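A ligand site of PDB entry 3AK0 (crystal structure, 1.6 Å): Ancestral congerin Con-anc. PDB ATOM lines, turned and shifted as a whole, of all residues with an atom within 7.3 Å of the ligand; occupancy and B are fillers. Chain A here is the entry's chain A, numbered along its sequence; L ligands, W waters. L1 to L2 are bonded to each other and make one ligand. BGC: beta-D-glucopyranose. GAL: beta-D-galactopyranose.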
ATOM      1  N   ARG A  30      -1.758   9.193 -17.438  1.00  0.00           N
ATOM      2  CA  ARG A  30      -0.698  10.200 -17.549  1.00  0.00           C
ATOM      3  C   ARG A  30      -0.100  10.216 -18.942  1.00  0.00           C
ATOM      4  O   ARG A  30      -0.169   9.226 -19.678  1.00  0.00           O
ATOM      5  CB  ARG A  30       0.431   9.923 -16.546  1.00  0.00           C
ATOM      6  CG  ARG A  30       1.203   8.631 -16.821  1.00  0.00           C
ATOM      7  CD  ARG A  30       2.423   8.569 -15.916  1.00  0.00           C
ATOM      8  NE  ARG A  30       3.123   7.309 -16.091  1.00  0.00           N
ATOM      9  CZ  ARG A  30       4.437   7.130 -15.879  1.00  0.00           C
ATOM     10  NH1 ARG A  30       4.991   5.933 -16.046  1.00  0.00           N
ATOM     11  NH2 ARG A  30       5.186   8.167 -15.496  1.00  0.00           N
ATOM     12  N   SER A  32       3.691  12.060 -20.815  1.00  0.00           N
ATOM     13  CA  SER A  32       4.800  12.999 -20.666  1.00  0.00           C
ATOM     14  C   SER A  32       5.326  13.571 -21.976  1.00  0.00           C
ATOM     15  O   SER A  32       5.243  12.917 -23.019  1.00  0.00           O
ATOM     16  CB  SER A  32       5.952  12.346 -19.868  1.00  0.00           C
ATOM     17  OG  SER A  32       6.455  11.194 -20.543  1.00  0.00           O
ATOM     18  N   ASN A  34       9.044  15.058 -23.303  1.00  0.00           N
ATOM     19  CA  ASN A  34      10.418  14.844 -22.871  1.00  0.00           C
ATOM     20  C   ASN A  34      11.354  15.507 -23.863  1.00  0.00           C
ATOM     21  O   ASN A  34      11.194  15.321 -25.072  1.00  0.00           O
ATOM     22  CB  ASN A  34      10.717  13.352 -22.859  1.00  0.00           C
ATOM     23  CG  ASN A  34       9.855  12.604 -21.897  1.00  0.00           C
ATOM     24  OD1 ASN A  34      10.192  12.488 -20.709  1.00  0.00           O
ATOM     25  ND2 ASN A  34       8.714  12.094 -22.382  1.00  0.00           N
ATOM     26  N   HIS A  45      11.737  16.257 -18.383  1.00  0.00           N
ATOM     27  CA  HIS A  45      10.572  15.348 -18.401  1.00  0.00           C
ATOM     28  C   HIS A  45       9.426  16.088 -17.722  1.00  0.00           C
ATOM     29  O   HIS A  45       9.564  16.529 -16.587  1.00  0.00           O
ATOM     30  CB  HIS A  45      10.993  14.088 -17.601  1.00  0.00           C
ATOM     31  CG  HIS A  45       9.883  13.129 -17.244  1.00  0.00           C
ATOM     32  ND1 HIS A  45       9.279  12.287 -18.165  1.00  0.00           N
ATOM     33  CD2 HIS A  45       9.341  12.817 -16.045  1.00  0.00           C
ATOM     34  CE1 HIS A  45       8.425  11.496 -17.533  1.00  0.00           C
ATOM     35  NE2 HIS A  45       8.429  11.810 -16.255  1.00  0.00           N
ATOM     36  N   ILE A  46       8.323  16.258 -18.453  1.00  0.00           N
ATOM     37  CA  ILE A  46       7.122  16.907 -17.922  1.00  0.00           C
ATOM     38  C   ILE A  46       6.052  15.829 -17.921  1.00  0.00           C
ATOM     39  O   ILE A  46       5.543  15.487 -18.978  1.00  0.00           O
ATOM     40  CB  ILE A  46       6.646  18.051 -18.825  1.00  0.00           C
ATOM     41  CG1 ILE A  46       7.825  18.949 -19.244  1.00  0.00           C
ATOM     42  CG2 ILE A  46       5.506  18.808 -18.110  1.00  0.00           C
ATOM     43  CD1 ILE A  46       7.512  19.747 -20.495  1.00  0.00           C
ATOM     44  N   ASP A  47       5.717  15.315 -16.742  1.00  0.00           N
ATOM     45  CA  ASP A  47       4.776  14.202 -16.670  1.00  0.00           C
ATOM     46  C   ASP A  47       3.462  14.751 -16.182  1.00  0.00           C
ATOM     47  O   ASP A  47       3.356  15.248 -15.073  1.00  0.00           O
ATOM     48  CB  ASP A  47       5.296  13.106 -15.719  1.00  0.00           C
ATOM     49  CG  ASP A  47       4.697  11.737 -16.004  1.00  0.00           C
ATOM     50  OD1 ASP A  47       4.225  11.488 -17.135  1.00  0.00           O
ATOM     51  OD2 ASP A  47       4.737  10.880 -15.090  1.00  0.00           O
ATOM     52  N   ARG A  49       0.179  14.074 -14.788  1.00  0.00           N
ATOM     53  CA  ARG A  49      -0.429  12.926 -14.074  1.00  0.00           C
ATOM     54  C   ARG A  49      -1.872  13.228 -13.690  1.00  0.00           C
ATOM     55  O   ARG A  49      -2.149  13.953 -12.716  1.00  0.00           O
ATOM     56  CB  ARG A  49       0.407  12.560 -12.849  1.00  0.00           C
ATOM     57  CG  ARG A  49       1.793  12.057 -13.282  1.00  0.00           C
ATOM     58  CD  ARG A  49       2.657  11.714 -12.050  1.00  0.00           C
ATOM     59  NE  ARG A  49       3.979  11.251 -12.492  1.00  0.00           N
ATOM     60  CZ  ARG A  49       4.929  10.739 -11.712  1.00  0.00           C
ATOM     61  NH1 ARG A  49       6.095  10.366 -12.269  1.00  0.00           N
ATOM     62  NH2 ARG A  49       4.754  10.598 -10.395  1.00  0.00           N
ATOM     63  N   TYR A  52      -1.849   8.907 -11.245  1.00  0.00           N
ATOM     64  CA  TYR A  52      -0.724   7.975 -11.197  1.00  0.00           C
ATOM     65  C   TYR A  52      -0.292   7.815  -9.781  1.00  0.00           C
ATOM     66  O   TYR A  52       0.519   8.563  -9.281  1.00  0.00           O
ATOM     67  CB  TYR A  52       0.426   8.441 -12.134  1.00  0.00           C
ATOM     68  CG  TYR A  52       1.635   7.539 -12.217  1.00  0.00           C
ATOM     69  CD1 TYR A  52       1.662   6.453 -13.105  1.00  0.00           C
ATOM     70  CD2 TYR A  52       2.766   7.777 -11.451  1.00  0.00           C
ATOM     71  CE1 TYR A  52       2.764   5.633 -13.208  1.00  0.00           C
ATOM     72  CE2 TYR A  52       3.900   6.935 -11.539  1.00  0.00           C
ATOM     73  CZ  TYR A  52       3.865   5.864 -12.434  1.00  0.00           C
ATOM     74  OH  TYR A  52       4.944   5.046 -12.556  1.00  0.00           O
ATOM     75  N   ALA A  54      -0.155   8.389  -6.007  1.00  0.00           N
ATOM     76  CA  ALA A  54      -0.442   9.530  -5.152  1.00  0.00           C
ATOM     77  C   ALA A  54      -0.590  10.847  -5.886  1.00  0.00           C
ATOM     78  O   ALA A  54      -1.074  11.823  -5.309  1.00  0.00           O
ATOM     79  CB  ALA A  54       0.639   9.643  -4.036  1.00  0.00           C
ATOM     80  N   ASP A  55      -0.219  10.876  -7.163  1.00  0.00           N
ATOM     81  CA  ASP A  55      -0.299  12.095  -7.952  1.00  0.00           C
ATOM     82  C   ASP A  55      -1.584  12.121  -8.748  1.00  0.00           C
ATOM     83  O   ASP A  55      -1.785  11.328  -9.679  1.00  0.00           O
ATOM     84  CB  ASP A  55       0.921  12.219  -8.871  1.00  0.00           C
ATOM     85  CG  ASP A  55       2.221  12.399  -8.109  1.00  0.00           C
ATOM     86  OD1 ASP A  55       2.274  13.303  -7.249  1.00  0.00           O
ATOM     87  OD2 ASP A  55       3.180  11.637  -8.338  1.00  0.00           O
ATOM     88  N   VAL A  60       4.603  16.381 -12.633  1.00  0.00           N
ATOM     89  CA  VAL A  60       5.888  15.981 -12.061  1.00  0.00           C
ATOM     90  C   VAL A  60       6.964  16.281 -13.095  1.00  0.00           C
ATOM     91  O   VAL A  60       6.876  15.843 -14.252  1.00  0.00           O
ATOM     92  CB  VAL A  60       5.890  14.482 -11.652  1.00  0.00           C
ATOM     93  CG1 VAL A  60       7.245  14.055 -11.125  1.00  0.00           C
ATOM     94  CG2 VAL A  60       4.826  14.232 -10.611  1.00  0.00           C
ATOM     95  N   LEU A  61       7.976  17.047 -12.675  1.00  0.00           N
ATOM     96  CA  LEU A  61       9.107  17.414 -13.560  1.00  0.00           C
ATOM     97  C   LEU A  61      10.354  16.732 -13.048  1.00  0.00           C
ATOM     98  O   LEU A  61      10.523  16.604 -11.835  1.00  0.00           O
ATOM     99  CB  LEU A  61       9.296  18.942 -13.580  1.00  0.00           C
ATOM    100  CG  LEU A  61       8.012  19.658 -14.023  1.00  0.00           C
ATOM    101  CD1 LEU A  61       7.280  20.208 -12.800  1.00  0.00           C
ATOM    102  CD2 LEU A  61       8.339  20.751 -15.007  1.00  0.00           C
ATOM    103  N   ASN A  62      11.177  16.217 -13.956  1.00  0.00           N
ATOM    104  CA  ASN A  62      12.456  15.606 -13.607  1.00  0.00           C
ATOM    105  C   ASN A  62      13.397  15.591 -14.813  1.00  0.00           C
ATOM    106  O   ASN A  62      13.059  16.049 -15.872  1.00  0.00           O
ATOM    107  CB  ASN A  62      12.220  14.160 -13.134  1.00  0.00           C
ATOM    108  CG  ASN A  62      13.250  13.696 -12.123  1.00  0.00           C
ATOM    109  OD1 ASN A  62      14.293  14.335 -11.952  1.00  0.00           O
ATOM    110  ND2 ASN A  62      12.955  12.562 -11.441  1.00  0.00           N
ATOM    111  N   SER A  63      14.590  15.067 -14.592  1.00  0.00           N
ATOM    112  CA  SER A  63      15.548  14.818 -15.654  1.00  0.00           C
ATOM    113  C   SER A  63      16.041  13.386 -15.471  1.00  0.00           C
ATOM    114  O   SER A  63      15.884  12.790 -14.387  1.00  0.00           O
ATOM    115  CB  SER A  63      16.710  15.818 -15.555  1.00  0.00           C
ATOM    116  OG  SER A  63      17.350  15.724 -14.278  1.00  0.00           O
ATOM    117  N   MET A  64      16.567  12.810 -16.553  1.00  0.00           N
ATOM    118  CA  MET A  64      17.070  11.447 -16.529  1.00  0.00           C
ATOM    119  C   MET A  64      18.472  11.464 -17.138  1.00  0.00           C
ATOM    120  O   MET A  64      18.700  12.020 -18.226  1.00  0.00           O
ATOM    121  CB  MET A  64      16.148  10.529 -17.320  1.00  0.00           C
ATOM    122  CG  MET A  64      16.785   9.182 -17.655  1.00  0.00           C
ATOM    123  SD  MET A  64      15.668   8.088 -18.573  1.00  0.00           S
ATOM    124  CE  MET A  64      14.843   7.249 -17.246  1.00  0.00           C
ATOM    125  N   TRP A  69      16.497   8.343 -13.129  1.00  0.00           N
ATOM    126  CA  TRP A  69      15.767   9.557 -12.757  1.00  0.00           C
ATOM    127  C   TRP A  69      16.482  10.348 -11.663  1.00  0.00           C
ATOM    128  O   TRP A  69      17.028   9.762 -10.716  1.00  0.00           O
ATOM    129  CB  TRP A  69      14.327   9.213 -12.343  1.00  0.00           C
ATOM    130  CG  TRP A  69      13.518   8.734 -13.492  1.00  0.00           C
ATOM    131  CD1 TRP A  69      13.029   7.464 -13.687  1.00  0.00           C
ATOM    132  CD2 TRP A  69      13.103   9.513 -14.612  1.00  0.00           C
ATOM    133  NE1 TRP A  69      12.308   7.417 -14.858  1.00  0.00           N
ATOM    134  CE2 TRP A  69      12.343   8.659 -15.454  1.00  0.00           C
ATOM    135  CE3 TRP A  69      13.287  10.854 -14.980  1.00  0.00           C
ATOM    136  CZ2 TRP A  69      11.780   9.103 -16.667  1.00  0.00           C
ATOM    137  CZ3 TRP A  69      12.712  11.304 -16.183  1.00  0.00           C
ATOM    138  CH2 TRP A  69      11.977  10.424 -17.005  1.00  0.00           C
ATOM    139  N   GLN A  70      16.423  11.678 -11.765  1.00  0.00           N
ATOM    140  CA  GLN A  70      17.006  12.560 -10.758  1.00  0.00           C
ATOM    141  C   GLN A  70      15.957  13.065  -9.735  1.00  0.00           C
ATOM    142  O   GLN A  70      15.019  12.335  -9.420  1.00  0.00           O
ATOM    143  CB  GLN A  70      17.779  13.663 -11.470  1.00  0.00           C
ATOM    144  CG  GLN A  70      18.727  13.082 -12.538  1.00  0.00           C
ATOM    145  CD  GLN A  70      19.841  12.252 -11.906  1.00  0.00           C
ATOM    146  OE1 GLN A  70      20.623  12.763 -11.095  1.00  0.00           O
ATOM    147  NE2 GLN A  70      19.918  10.945 -12.269  1.00  0.00           N
ATOM    148  N   GLN A  71      16.139  14.274  -9.204  1.00  0.00           N
ATOM    149  CA  GLN A  71      15.231  14.796  -8.205  1.00  0.00           C
ATOM    150  C   GLN A  71      13.949  15.356  -8.810  1.00  0.00           C
ATOM    151  O   GLN A  71      14.009  16.245  -9.657  1.00  0.00           O
ATOM    152  CB  GLN A  71      15.929  15.911  -7.411  1.00  0.00           C
ATOM    153  CG  GLN A  71      15.072  16.410  -6.252  1.00  0.00           C
ATOM    154  CD  GLN A  71      15.677  17.612  -5.494  1.00  0.00           C
ATOM    155  OE1 GLN A  71      16.122  18.610  -6.104  1.00  0.00           O
ATOM    156  NE2 GLN A  71      15.644  17.543  -4.158  1.00  0.00           N
ATOM    157  N   GLU A  72      12.801  14.869  -8.348  1.00  0.00           N
ATOM    158  CA  GLU A  72      11.502  15.392  -8.796  1.00  0.00           C
ATOM    159  C   GLU A  72      11.150  16.771  -8.237  1.00  0.00           C
ATOM    160  O   GLU A  72      11.526  17.140  -7.111  1.00  0.00           O
ATOM    161  CB  GLU A  72      10.360  14.414  -8.425  1.00  0.00           C
ATOM    162  CG  GLU A  72      10.510  13.089  -9.108  1.00  0.00           C
ATOM    163  CD  GLU A  72       9.461  12.090  -8.698  1.00  0.00           C
ATOM    164  OE1 GLU A  72       8.841  12.184  -7.614  1.00  0.00           O
ATOM    165  OE2 GLU A  72       9.302  11.138  -9.470  1.00  0.00           O
ATOM    166  N   GLN A  73      10.380  17.509  -9.047  1.00  0.00           N
ATOM    167  CA  GLN A  73       9.683  18.726  -8.626  1.00  0.00           C
ATOM    168  C   GLN A  73       8.230  18.615  -9.043  1.00  0.00           C
ATOM    169  O   GLN A  73       7.918  18.007 -10.064  1.00  0.00           O
ATOM    170  CB  GLN A  73      10.299  19.982  -9.270  1.00  0.00           C
ATOM    171  CG  GLN A  73      11.751  20.249  -8.848  1.00  0.00           C
ATOM    172  CD  GLN A  73      12.265  21.634  -9.232  1.00  0.00           C
ATOM    173  OE1 GLN A  73      11.601  22.402  -9.963  1.00  0.00           O
ATOM    174  NE2 GLN A  73      13.457  21.972  -8.718  1.00  0.00           N
ATOM    175  N   ARG A  74       7.323  19.157  -8.256  1.00  0.00           N
ATOM    176  CA  ARG A  74       5.900  19.049  -8.579  1.00  0.00           C
ATOM    177  C   ARG A  74       5.261  20.405  -8.743  1.00  0.00           C
ATOM    178  O   ARG A  74       5.733  21.402  -8.176  1.00  0.00           O
ATOM    179  CB  ARG A  74       5.151  18.245  -7.498  1.00  0.00           C
ATOM    180  CG  ARG A  74       5.293  16.740  -7.675  1.00  0.00           C
ATOM    181  CD  ARG A  74       4.910  15.895  -6.451  1.00  0.00           C
ATOM    182  NE  ARG A  74       4.927  14.485  -6.832  1.00  0.00           N
ATOM    183  CZ  ARG A  74       6.006  13.732  -6.952  1.00  0.00           C
ATOM    184  NH1 ARG A  74       7.207  14.221  -6.659  1.00  0.00           N
ATOM    185  NH2 ARG A  74       5.887  12.472  -7.356  1.00  0.00           N
HETATM  186  C2  BGC L   1       7.610   8.588  -7.188  1.00  0.00           C
HETATM  187  C3  BGC L   1       7.186   8.479  -8.655  1.00  0.00           C
HETATM  188  C4  BGC L   1       8.134   7.625  -9.501  1.00  0.00           C
HETATM  189  C5  BGC L   1       8.202   6.260  -8.809  1.00  0.00           C
HETATM  190  C6  BGC L   1       9.204   5.346  -9.456  1.00  0.00           C
HETATM  191  C1  BGC L   1       7.782   7.185  -6.643  1.00  0.00           C
HETATM  192  O1  BGC L   1       8.409   7.271  -5.383  1.00  0.00           O
HETATM  193  O2  BGC L   1       6.612   9.291  -6.450  1.00  0.00           O
HETATM  194  O3  BGC L   1       7.075   9.768  -9.212  1.00  0.00           O
HETATM  195  O4  BGC L   1       7.560   7.465 -10.792  1.00  0.00           O
HETATM  196  O5  BGC L   1       8.643   6.456  -7.466  1.00  0.00           O
HETATM  197  O6  BGC L   1      10.456   5.972  -9.363  1.00  0.00           O
HETATM  198  C1  GAL L   2       8.462   7.686 -11.868  1.00  0.00           C
HETATM  199  C2  GAL L   2       7.799   7.156 -13.143  1.00  0.00           C
HETATM  200  C3  GAL L   2       8.661   7.508 -14.354  1.00  0.00           C
HETATM  201  C4  GAL L   2       8.936   8.998 -14.371  1.00  0.00           C
HETATM  202  C5  GAL L   2       9.577   9.405 -13.032  1.00  0.00           C
HETATM  203  C6  GAL L   2       9.832  10.902 -12.947  1.00  0.00           C
HETATM  204  O2  GAL L   2       7.599   5.745 -13.133  1.00  0.00           O
HETATM  205  O3  GAL L   2       7.985   7.072 -15.514  1.00  0.00           O
HETATM  206  O4  GAL L   2       7.724   9.701 -14.596  1.00  0.00           O
HETATM  207  O5  GAL L   2       8.677   9.073 -11.981  1.00  0.00           O
HETATM  208  O6  GAL L   2      10.565  11.159 -11.756  1.00  0.00           O
HETATM  209  O   HOH W   1       8.250   4.653 -16.242  1.00  0.00           O
HETATM  210  O   HOH W   2       7.532   8.154 -18.149  1.00  0.00           O
HETATM  211  O   HOH W   3      11.962   4.527 -11.402  1.00  0.00           O
HETATM  212  O   HOH W   4       9.967   4.257 -13.252  1.00  0.00           O
HETATM  213  O   HOH W   5      11.807   8.813  -9.987  1.00  0.00           O
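Water W5 lies within hydrogen-bond range of O6 of GAL L2 (3.2 Å) and OE2 of Glu 72 (3.5 Å).
Residues that only touch the ligand: Trp 69 (3.6 Å).
Within 4 Å of the ligand: Arg 30, His 45, Asp 47, Arg 49, Tyr 52, Asn 62, Trp 69, Glu 72 and Arg 74.
OD2 of Asp 47 lies within salt-bridge range of NE of Arg 49 (2.7 Å).
OD2 of Asp 55 is in salt-bridge range of NH2 of Arg 49 (2.8 Å).
The side-chain amide oxygen (OD1) of Asn 34 lies within hydrogen-bond range of a ring nitrogen (ND1) of His 45, 2.7 Å away.
The backbone carbonyl oxygen of Gln 70 is in hydrogen-bond range of the side-chain amide nitrogen of Asn 62 (2.9 Å).
O of Gln 71 lies close to OD1 of Asn 62 (3.0 Å).
OD2 of Asp 47 lies within salt-bridge range of NH2 of Arg 30, at 2.8 Å.
The backbone carbonyl oxygen (O) of Val 60 lies within hydrogen-bond range of the backbone NH (N) of Asp 47 (2.8 Å).
NE of Arg 74 is in salt-bridge range of OD1 of Asp 55 (2.9 Å).
The side-chain carboxylate (OE2) of Glu 72 sits at hydrogen-bond distance from an oxygen (O6) of GAL L2.
An oxygen (O3) of BGC L1 lies within hydrogen-bond range of the guanidinium group (NH2) of Arg 49.
A ring nitrogen (NE2) of His 45 sits at hydrogen-bond distance from an oxygen (O4) of GAL L2 (2.8 Å).
ND2 of Asn 62 lies within hydrogen-bond range of O6 of GAL L2.
OH of Tyr 52 sits at hydrogen-bond distance from O2 of GAL L2 (2.8 Å).
O3 of GAL L2 is in hydrogen-bond range of NH2 of Arg 30 (3.0 Å).
O4 of GAL L2 lies within hydrogen-bond range of OD2 of Asp 47 (3.2 Å).
The guanidinium group (NH2) of Arg 74 lies within hydrogen-bond range of an oxygen (O2) of BGC L1 (3.4 Å).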
